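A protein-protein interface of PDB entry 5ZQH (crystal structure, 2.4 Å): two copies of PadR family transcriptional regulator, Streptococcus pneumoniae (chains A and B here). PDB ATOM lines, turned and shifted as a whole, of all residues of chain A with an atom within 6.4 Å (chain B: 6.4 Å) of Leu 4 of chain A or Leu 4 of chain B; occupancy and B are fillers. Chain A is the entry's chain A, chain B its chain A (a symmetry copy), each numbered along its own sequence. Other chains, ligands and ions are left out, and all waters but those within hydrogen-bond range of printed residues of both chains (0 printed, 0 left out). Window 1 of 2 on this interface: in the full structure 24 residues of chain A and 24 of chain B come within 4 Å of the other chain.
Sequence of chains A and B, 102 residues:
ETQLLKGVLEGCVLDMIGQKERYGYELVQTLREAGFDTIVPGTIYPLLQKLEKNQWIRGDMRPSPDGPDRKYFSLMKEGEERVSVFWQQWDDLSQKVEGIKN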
ATOM      1  N   THR A   2      -7.661  -8.952  11.550  1.00  0.00           N
ATOM      2  CA  THR A   2      -7.294  -7.978  12.601  1.00  0.00           C
ATOM      3  C   THR A   2      -7.511  -6.522  12.181  1.00  0.00           C
ATOM      4  O   THR A   2      -7.592  -6.221  10.983  1.00  0.00           O
ATOM      5  CB  THR A   2      -5.827  -8.141  13.080  1.00  0.00           C
ATOM      6  OG1 THR A   2      -4.927  -7.889  11.994  1.00  0.00           O
ATOM      7  CG2 THR A   2      -5.571  -9.537  13.658  1.00  0.00           C
ATOM      8  N   GLN A   3      -7.592  -5.631  13.179  1.00  0.00           N
ATOM      9  CA  GLN A   3      -7.742  -4.183  12.962  1.00  0.00           C
ATOM     10  C   GLN A   3      -6.607  -3.590  12.134  1.00  0.00           C
ATOM     11  O   GLN A   3      -6.849  -2.737  11.271  1.00  0.00           O
ATOM     12  CB  GLN A   3      -7.851  -3.431  14.289  1.00  0.00           C
ATOM     13  CG  GLN A   3      -9.220  -3.499  14.949  1.00  0.00           C
ATOM     14  CD  GLN A   3      -9.216  -2.920  16.354  1.00  0.00           C
ATOM     15  OE1 GLN A   3      -8.432  -3.334  17.215  1.00  0.00           O
ATOM     16  NE2 GLN A   3     -10.100  -1.959  16.595  1.00  0.00           N
ATOM     17  N   LEU A   4      -5.383  -4.049  12.406  1.00  0.00           N
ATOM     18  CA  LEU A   4      -4.194  -3.656  11.645  1.00  0.00           C
ATOM     19  C   LEU A   4      -4.325  -4.006  10.159  1.00  0.00           C
ATOM     20  O   LEU A   4      -4.111  -3.141   9.300  1.00  0.00           O
ATOM     21  CB  LEU A   4      -2.919  -4.271  12.252  1.00  0.00           C
ATOM     22  CG  LEU A   4      -1.582  -4.233  11.492  1.00  0.00           C
ATOM     23  CD1 LEU A   4      -1.041  -2.821  11.284  1.00  0.00           C
ATOM     24  CD2 LEU A   4      -0.557  -5.106  12.201  1.00  0.00           C
ATOM     25  N   LEU A   5      -4.690  -5.261   9.876  1.00  0.00           N
ATOM     26  CA  LEU A   5      -4.844  -5.755   8.509  1.00  0.00           C
ATOM     27  C   LEU A   5      -5.877  -4.952   7.721  1.00  0.00           C
ATOM     28  O   LEU A   5      -5.603  -4.540   6.593  1.00  0.00           O
ATOM     29  CB  LEU A   5      -5.155  -7.267   8.482  1.00  0.00           C
ATOM     30  CG  LEU A   5      -5.238  -8.025   7.139  1.00  0.00           C
ATOM     31  CD1 LEU A   5      -3.964  -7.900   6.313  1.00  0.00           C
ATOM     32  CD2 LEU A   5      -5.574  -9.494   7.357  1.00  0.00           C
ATOM     33  N   LYS A   6      -7.039  -4.719   8.336  1.00  0.00           N
ATOM     34  CA  LYS A   6      -8.119  -3.912   7.748  1.00  0.00           C
ATOM     35  C   LYS A   6      -7.674  -2.488   7.424  1.00  0.00           C
ATOM     36  O   LYS A   6      -7.995  -1.967   6.357  1.00  0.00           O
ATOM     37  CB  LYS A   6      -9.344  -3.888   8.666  1.00  0.00           C
ATOM     38  CG  LYS A   6     -10.252  -5.092   8.517  1.00  0.00           C
ATOM     39  CD  LYS A   6     -11.028  -5.356   9.798  1.00  0.00           C
ATOM     40  CE  LYS A   6     -12.038  -6.476   9.600  1.00  0.00           C
ATOM     41  NZ  LYS A   6     -12.671  -6.878  10.887  1.00  0.00           N
ATOM     42  N   GLY A   7      -6.928  -1.881   8.345  1.00  0.00           N
ATOM     43  CA  GLY A   7      -6.374  -0.543   8.161  1.00  0.00           C
ATOM     44  C   GLY A   7      -5.422  -0.467   6.983  1.00  0.00           C
ATOM     45  O   GLY A   7      -5.468   0.495   6.209  1.00  0.00           O
ATOM     46  N   VAL A   8      -4.577  -1.493   6.841  1.00  0.00           N
ATOM     47  CA  VAL A   8      -3.599  -1.557   5.748  1.00  0.00           C
ATOM     48  C   VAL A   8      -4.277  -1.699   4.374  1.00  0.00           C
ATOM     49  O   VAL A   8      -4.011  -0.867   3.484  1.00  0.00           O
ATOM     50  CB  VAL A   8      -2.478  -2.607   5.992  1.00  0.00           C
ATOM     51  CG1 VAL A   8      -1.645  -2.839   4.737  1.00  0.00           C
ATOM     52  CG2 VAL A   8      -1.575  -2.159   7.132  1.00  0.00           C
ATOM     53  N   LEU A   9      -5.150  -2.704   4.197  1.00  0.00           N
ATOM     54  CA  LEU A   9      -5.855  -2.841   2.907  1.00  0.00           C
ATOM     55  C   LEU A   9      -6.752  -1.664   2.538  1.00  0.00           C
ATOM     56  O   LEU A   9      -6.909  -1.384   1.349  1.00  0.00           O
ATOM     57  CB  LEU A   9      -6.549  -4.198   2.645  1.00  0.00           C
ATOM     58  CG  LEU A   9      -7.214  -5.177   3.603  1.00  0.00           C
ATOM     59  CD1 LEU A   9      -8.493  -5.744   2.993  1.00  0.00           C
ATOM     60  CD2 LEU A   9      -6.239  -6.305   3.872  1.00  0.00           C
ATOM     61  N   PHE A  86      -3.512   8.425   5.378  1.00  0.00           N
ATOM     62  CA  PHE A  86      -2.935   7.074   5.455  1.00  0.00           C
ATOM     63  C   PHE A  86      -1.407   7.054   5.376  1.00  0.00           C
ATOM     64  O   PHE A  86      -0.762   6.423   6.218  1.00  0.00           O
ATOM     65  CB  PHE A  86      -3.538   6.125   4.400  1.00  0.00           C
ATOM     66  CG  PHE A  86      -2.768   4.830   4.238  1.00  0.00           C
ATOM     67  CD1 PHE A  86      -2.853   3.822   5.204  1.00  0.00           C
ATOM     68  CD2 PHE A  86      -1.940   4.628   3.130  1.00  0.00           C
ATOM     69  CE1 PHE A  86      -2.132   2.642   5.066  1.00  0.00           C
ATOM     70  CE2 PHE A  86      -1.220   3.449   2.985  1.00  0.00           C
ATOM     71  CZ  PHE A  86      -1.317   2.455   3.956  1.00  0.00           C
ATOM     72  N   GLN A  89       0.091   8.701   8.432  1.00  0.00           N
ATOM     73  CA  GLN A  89      -0.112   7.780   9.553  1.00  0.00           C
ATOM     74  C   GLN A  89       0.765   6.531   9.446  1.00  0.00           C
ATOM     75  O   GLN A  89       1.247   6.037  10.458  1.00  0.00           O
ATOM     76  CB  GLN A  89      -1.583   7.393   9.694  1.00  0.00           C
ATOM     77  CG  GLN A  89      -1.959   6.961  11.101  1.00  0.00           C
ATOM     78  CD  GLN A  89      -3.456   6.858  11.323  1.00  0.00           C
ATOM     79  OE1 GLN A  89      -3.978   7.382  12.305  1.00  0.00           O
ATOM     80  NE2 GLN A  89      -4.153   6.175  10.418  1.00  0.00           N
ATOM     81  N   TRP A  90       0.976   6.038   8.226  1.00  0.00           N
ATOM     82  CA  TRP A  90       1.852   4.887   8.011  1.00  0.00           C
ATOM     83  C   TRP A  90       3.319   5.223   8.314  1.00  0.00           C
ATOM     84  O   TRP A  90       3.990   4.449   9.005  1.00  0.00           O
ATOM     85  CB  TRP A  90       1.703   4.280   6.607  1.00  0.00           C
ATOM     86  CG  TRP A  90       2.605   3.104   6.431  1.00  0.00           C
ATOM     87  CD1 TRP A  90       3.805   3.078   5.764  1.00  0.00           C
ATOM     88  CD2 TRP A  90       2.420   1.794   6.978  1.00  0.00           C
ATOM     89  NE1 TRP A  90       4.364   1.822   5.843  1.00  0.00           N
ATOM     90  CE2 TRP A  90       3.538   1.013   6.581  1.00  0.00           C
ATOM     91  CE3 TRP A  90       1.413   1.196   7.754  1.00  0.00           C
ATOM     92  CZ2 TRP A  90       3.677  -0.336   6.936  1.00  0.00           C
ATOM     93  CZ3 TRP A  90       1.548  -0.147   8.104  1.00  0.00           C
ATOM     94  CH2 TRP A  90       2.679  -0.898   7.694  1.00  0.00           C
ATOM     95  N   LEU A  93       3.582   5.782  12.288  1.00  0.00           N
ATOM     96  CA  LEU A  93       3.500   4.546  13.068  1.00  0.00           C
ATOM     97  C   LEU A  93       4.670   3.587  12.817  1.00  0.00           C
ATOM     98  O   LEU A  93       5.081   2.876  13.735  1.00  0.00           O
ATOM     99  CB  LEU A  93       2.139   3.852  12.885  1.00  0.00           C
ATOM    100  CG  LEU A  93       0.886   4.595  13.390  1.00  0.00           C
ATOM    101  CD1 LEU A  93      -0.384   3.939  12.864  1.00  0.00           C
ATOM    102  CD2 LEU A  93       0.846   4.704  14.909  1.00  0.00           C
ATOM    103  N   THR B   2      -8.503   5.638  13.665  1.00  0.00           N
ATOM    104  CA  THR B   2      -8.578   4.693  12.529  1.00  0.00           C
ATOM    105  C   THR B   2      -8.270   3.246  12.923  1.00  0.00           C
ATOM    106  O   THR B   2      -7.648   2.999  13.964  1.00  0.00           O
ATOM    107  CB  THR B   2      -7.646   5.095  11.356  1.00  0.00           C
ATOM    108  OG1 THR B   2      -6.280   5.069  11.786  1.00  0.00           O
ATOM    109  CG2 THR B   2      -7.994   6.482  10.805  1.00  0.00           C
ATOM    110  N   GLN B   3      -8.702   2.304  12.074  1.00  0.00           N
ATOM    111  CA  GLN B   3      -8.449   0.867  12.261  1.00  0.00           C
ATOM    112  C   GLN B   3      -6.962   0.535  12.330  1.00  0.00           C
ATOM    113  O   GLN B   3      -6.550  -0.301  13.143  1.00  0.00           O
ATOM    114  CB  GLN B   3      -9.105   0.039  11.155  1.00  0.00           C
ATOM    115  CG  GLN B   3     -10.600  -0.179  11.324  1.00  0.00           C
ATOM    116  CD  GLN B   3     -11.235  -0.821  10.102  1.00  0.00           C
ATOM    117  OE1 GLN B   3     -11.117  -0.317   8.979  1.00  0.00           O
ATOM    118  NE2 GLN B   3     -11.920  -1.938  10.315  1.00  0.00           N
ATOM    119  N   LEU B   4      -6.174   1.195  11.476  1.00  0.00           N
ATOM    120  CA  LEU B   4      -4.716   1.066  11.470  1.00  0.00           C
ATOM    121  C   LEU B   4      -4.101   1.463  12.817  1.00  0.00           C
ATOM    122  O   LEU B   4      -3.312   0.699  13.384  1.00  0.00           O
ATOM    123  CB  LEU B   4      -4.092   1.870  10.314  1.00  0.00           C
ATOM    124  CG  LEU B   4      -2.576   2.116  10.247  1.00  0.00           C
ATOM    125  CD1 LEU B   4      -1.759   0.840  10.063  1.00  0.00           C
ATOM    126  CD2 LEU B   4      -2.260   3.123   9.151  1.00  0.00           C
ATOM    127  N   LEU B   5      -4.482   2.644  13.315  1.00  0.00           N
ATOM    128  CA  LEU B   5      -3.977   3.173  14.581  1.00  0.00           C
ATOM    129  C   LEU B   5      -4.269   2.238  15.752  1.00  0.00           C
ATOM    130  O   LEU B   5      -3.370   1.943  16.541  1.00  0.00           O
ATOM    131  CB  LEU B   5      -4.496   4.603  14.847  1.00  0.00           C
ATOM    132  CG  LEU B   5      -3.992   5.402  16.068  1.00  0.00           C
ATOM    133  CD1 LEU B   5      -2.476   5.556  16.087  1.00  0.00           C
ATOM    134  CD2 LEU B   5      -4.654   6.772  16.140  1.00  0.00           C
ATOM    135  N   LYS B   6      -5.515   1.765  15.834  1.00  0.00           N
ATOM    136  CA  LYS B   6      -5.951   0.807  16.861  1.00  0.00           C
ATOM    137  C   LYS B   6      -5.153  -0.493  16.825  1.00  0.00           C
ATOM    138  O   LYS B   6      -4.758  -1.007  17.870  1.00  0.00           O
ATOM    139  CB  LYS B   6      -7.449   0.511  16.731  1.00  0.00           C
ATOM    140  CG  LYS B   6      -8.341   1.536  17.401  1.00  0.00           C
ATOM    141  CD  LYS B   6      -9.710   1.586  16.741  1.00  0.00           C
ATOM    142  CE  LYS B   6     -10.647   2.511  17.503  1.00  0.00           C
ATOM    143  NZ  LYS B   6     -11.925   2.723  16.769  1.00  0.00           N
ATOM    144  N   GLY B   7      -4.910  -1.002  15.618  1.00  0.00           N
ATOM    145  CA  GLY B   7      -4.110  -2.205  15.410  1.00  0.00           C
ATOM    146  C   GLY B   7      -2.684  -2.043  15.900  1.00  0.00           C
ATOM    147  O   GLY B   7      -2.137  -2.956  16.528  1.00  0.00           O
ATOM    148  N   VAL B   8      -2.096  -0.874  15.626  1.00  0.00           N
ATOM    149  CA  VAL B   8      -0.718  -0.576  16.038  1.00  0.00           C
ATOM    150  C   VAL B   8      -0.579  -0.488  17.568  1.00  0.00           C
ATOM    151  O   VAL B   8       0.264  -1.209  18.137  1.00  0.00           O
ATOM    152  CB  VAL B   8      -0.110   0.647  15.294  1.00  0.00           C
ATOM    153  CG1 VAL B   8       1.202   1.093  15.927  1.00  0.00           C
ATOM    154  CG2 VAL B   8       0.117   0.311  13.827  1.00  0.00           C
ATOM    155  N   LEU B   9      -1.391   0.350  18.233  1.00  0.00           N
ATOM    156  CA  LEU B   9      -1.319   0.424  19.706  1.00  0.00           C
ATOM    157  C   LEU B   9      -1.652  -0.876  20.431  1.00  0.00           C
ATOM    158  O   LEU B   9      -1.101  -1.117  21.506  1.00  0.00           O
ATOM    159  CB  LEU B   9      -2.002   1.643  20.366  1.00  0.00           C
ATOM    160  CG  LEU B   9      -3.238   2.432  19.959  1.00  0.00           C
ATOM    161  CD1 LEU B   9      -4.079   2.788  21.182  1.00  0.00           C
ATOM    162  CD2 LEU B   9      -2.778   3.704  19.275  1.00  0.00           C
ATOM    163  N   PHE B  86       1.369 -10.341  15.778  1.00  0.00           N
ATOM    164  CA  PHE B  86       1.560  -8.914  15.479  1.00  0.00           C
ATOM    165  C   PHE B  86       2.865  -8.611  14.738  1.00  0.00           C
ATOM    166  O   PHE B  86       2.839  -7.919  13.718  1.00  0.00           O
ATOM    167  CB  PHE B  86       1.447  -8.036  16.742  1.00  0.00           C
ATOM    168  CG  PHE B  86       1.934  -6.616  16.540  1.00  0.00           C
ATOM    169  CD1 PHE B  86       1.168  -5.692  15.820  1.00  0.00           C
ATOM    170  CD2 PHE B  86       3.169  -6.208  17.050  1.00  0.00           C
ATOM    171  CE1 PHE B  86       1.623  -4.395  15.618  1.00  0.00           C
ATOM    172  CE2 PHE B  86       3.627  -4.911  16.854  1.00  0.00           C
ATOM    173  CZ  PHE B  86       2.852  -4.005  16.136  1.00  0.00           C
ATOM    174  N   GLN B  89       2.789 -10.116  11.270  1.00  0.00           N
ATOM    175  CA  GLN B  89       1.859  -9.308  10.478  1.00  0.00           C
ATOM    176  C   GLN B  89       2.415  -7.917  10.170  1.00  0.00           C
ATOM    177  O   GLN B  89       2.189  -7.397   9.083  1.00  0.00           O
ATOM    178  CB  GLN B  89       0.496  -9.204  11.157  1.00  0.00           C
ATOM    179  CG  GLN B  89      -0.640  -8.923  10.188  1.00  0.00           C
ATOM    180  CD  GLN B  89      -2.016  -9.106  10.798  1.00  0.00           C
ATOM    181  OE1 GLN B  89      -2.873  -9.767  10.214  1.00  0.00           O
ATOM    182  NE2 GLN B  89      -2.239  -8.515  11.969  1.00  0.00           N
ATOM    183  N   TRP B  90       3.146  -7.329  11.117  1.00  0.00           N
ATOM    184  CA  TRP B  90       3.776  -6.029  10.896  1.00  0.00           C
ATOM    185  C   TRP B  90       4.892  -6.106   9.845  1.00  0.00           C
ATOM    186  O   TRP B  90       4.941  -5.261   8.947  1.00  0.00           O
ATOM    187  CB  TRP B  90       4.284  -5.385  12.196  1.00  0.00           C
ATOM    188  CG  TRP B  90       4.911  -4.057  11.930  1.00  0.00           C
ATOM    189  CD1 TRP B  90       6.253  -3.777  11.861  1.00  0.00           C
ATOM    190  CD2 TRP B  90       4.229  -2.833  11.634  1.00  0.00           C
ATOM    191  NE1 TRP B  90       6.446  -2.446  11.565  1.00  0.00           N
ATOM    192  CE2 TRP B  90       5.224  -1.842  11.419  1.00  0.00           C
ATOM    193  CE3 TRP B  90       2.876  -2.471  11.541  1.00  0.00           C
ATOM    194  CZ2 TRP B  90       4.905  -0.510  11.117  1.00  0.00           C
ATOM    195  CZ3 TRP B  90       2.557  -1.146  11.244  1.00  0.00           C
ATOM    196  CH2 TRP B  90       3.574  -0.180  11.032  1.00  0.00           C
ATOM    197  N   LEU B  93       3.109  -6.817   6.312  1.00  0.00           N
ATOM    198  CA  LEU B  93       2.403  -5.660   5.759  1.00  0.00           C
ATOM    199  C   LEU B  93       3.329  -4.492   5.404  1.00  0.00           C
ATOM    200  O   LEU B  93       3.055  -3.767   4.446  1.00  0.00           O
ATOM    201  CB  LEU B  93       1.245  -5.217   6.672  1.00  0.00           C
ATOM    202  CG  LEU B  93       0.075  -6.201   6.869  1.00  0.00           C
ATOM    203  CD1 LEU B  93      -0.819  -5.761   8.021  1.00  0.00           C
ATOM    204  CD2 LEU B  93      -0.743  -6.396   5.598  1.00  0.00           C
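The side-chain hydroxyl (OG1) of Thr 2 of chain A is in hydrogen-bond range of the side-chain amide nitrogen (NE2) of Gln 89 of chain B (2.8 Å).
NE2 of Gln 89 of chain A sits at hydrogen-bond distance from OG1 of Thr 2 of chain B (2.8 Å).
The backbone carbonyl oxygen (O) of Gln 3 of chain A sits close to the backbone carbonyl oxygen (O) of Gln 3 of chain B, at 3.1 Å.
The side-chain hydroxyl (OG1) of Thr 2 of chain A sits at hydrogen-bond distance from the backbone NH (N) of Leu 5 of chain A, 3.4 Å away.
The backbone NH (N) of Leu 5 of chain B sits at hydrogen-bond distance from the side-chain hydroxyl (OG1) of Thr 2 of chain B, 3.4 Å away.
Among the printed residues, merely in contact across the chains: Gln 3 of chain A with Leu 4 of chain B, Gln 3 of chain A with Lys 6 of chain B, Leu 4 of chain A with Gln 3 of chain B, Leu 4 of chain A with Leu 4 of chain B, Leu 4 of chain A with Gly 7 of chain B, Leu 4 of chain A with Gln 89 of chain B, Leu 4 of chain A with Trp 90 of chain B, Leu 4 of chain A with Leu 93 of chain B, Leu 5 of chain A with Gln 89 of chain B, Leu 5 of chain A with Leu 93 of chain B, Lys 6 of chain A with Gln 3 of chain B, Gly 7 of chain A with Leu 4 of chain B, Val 8 of chain A with Leu 93 of chain B, Gln 89 of chain A with Leu 4 of chain B, Gln 89 of chain A with Leu 5 of chain B, Trp 90 of chain A with Leu 4 of chain B, Trp 90 of chain A with Trp 90 of chain B, Leu 93 of chain A with Leu 4 of chain B, Leu 93 of chain A with Leu 5 of chain B and Leu 93 of chain A with Val 8 of chain B.
Printed residues of chain B within 4 Å of Gly 7 of chain A: Leu 4 (3.7 Å).
Phe 86 of chain A touches none of the printed residues of chain B.
Printed residues of chain B within 4 Å of Gln 89 of chain A: Thr 2, Leu 4 and Leu 5.
Of the printed residues of chain A, Thr 2 of chain B touches Gln 89 (2.8 Å).
Printed residues of chain A within 4 Å of Leu 4 of chain B: Gln 3 (3.99 Å), Leu 4 (3.9 Å), Gly 7 (3.7 Å), Gln 89 (3.8 Å), Trp 90 (3.9 Å) and Leu 93 (3.9 Å).
Printed residues of chain A within 4 Å of Leu 5 of chain B: Gln 89 (3.8 Å) and Leu 93 (3.6 Å).
Phe 86 of chain B touches none of the printed residues of chain A.
The nearest printed residue of chain B that does not touch Leu 4 of chain A is Phe 86 of chain B (4.1 Å).
The nearest printed residue of chain A that does not touch Leu 4 of chain B is Phe 86 of chain A (4.1 Å).
The nearest printed residue of chain A that does not touch Gly 7 of chain B is Gln 3 of chain A (4.04 Å).
Of the 12 printed residues of chain B, 10 touch a printed residue of chain A.
Printed residues of chain B that touch a printed residue of chain A: Thr 2, Gln 3, Leu 4, Leu 5, Lys 6, Gly 7, Val 8, Gln 89, Trp 90 and Leu 93.
Hydrophobic or aromatic side chains of chain B within 4 Å of the printed part of chain A: Leu 4, Leu 5, Val 8, Trp 90 and Leu 93.
Among the printed residues, 23 pairs touch across the chains.
Thr 2 of chain A touches Gln 89 of chain B, and with the chains exchanged Gln 89 of chain A touches Thr 2 of chain B.
Leu 4 of chain A touches Trp 90 of chain B, and with the chains exchanged Trp 90 of chain A touches Leu 4 of chain B.
Leu 4 of chain A touches Leu 93 of chain B, and with the chains exchanged Leu 93 of chain A touches Leu 4 of chain B.
Leu 5 of chain A touches Gln 89 of chain B, and with the chains exchanged Gln 89 of chain A touches Leu 5 of chain B.
Positions printed for both chains: 2, 3, 4, 5, 6, 7, 8, 9, 86, 89, 90 and 93.
Of the 23 pairs that touch across the chains among the printed residues, 23 have their exchanged pair printed and touching as well.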
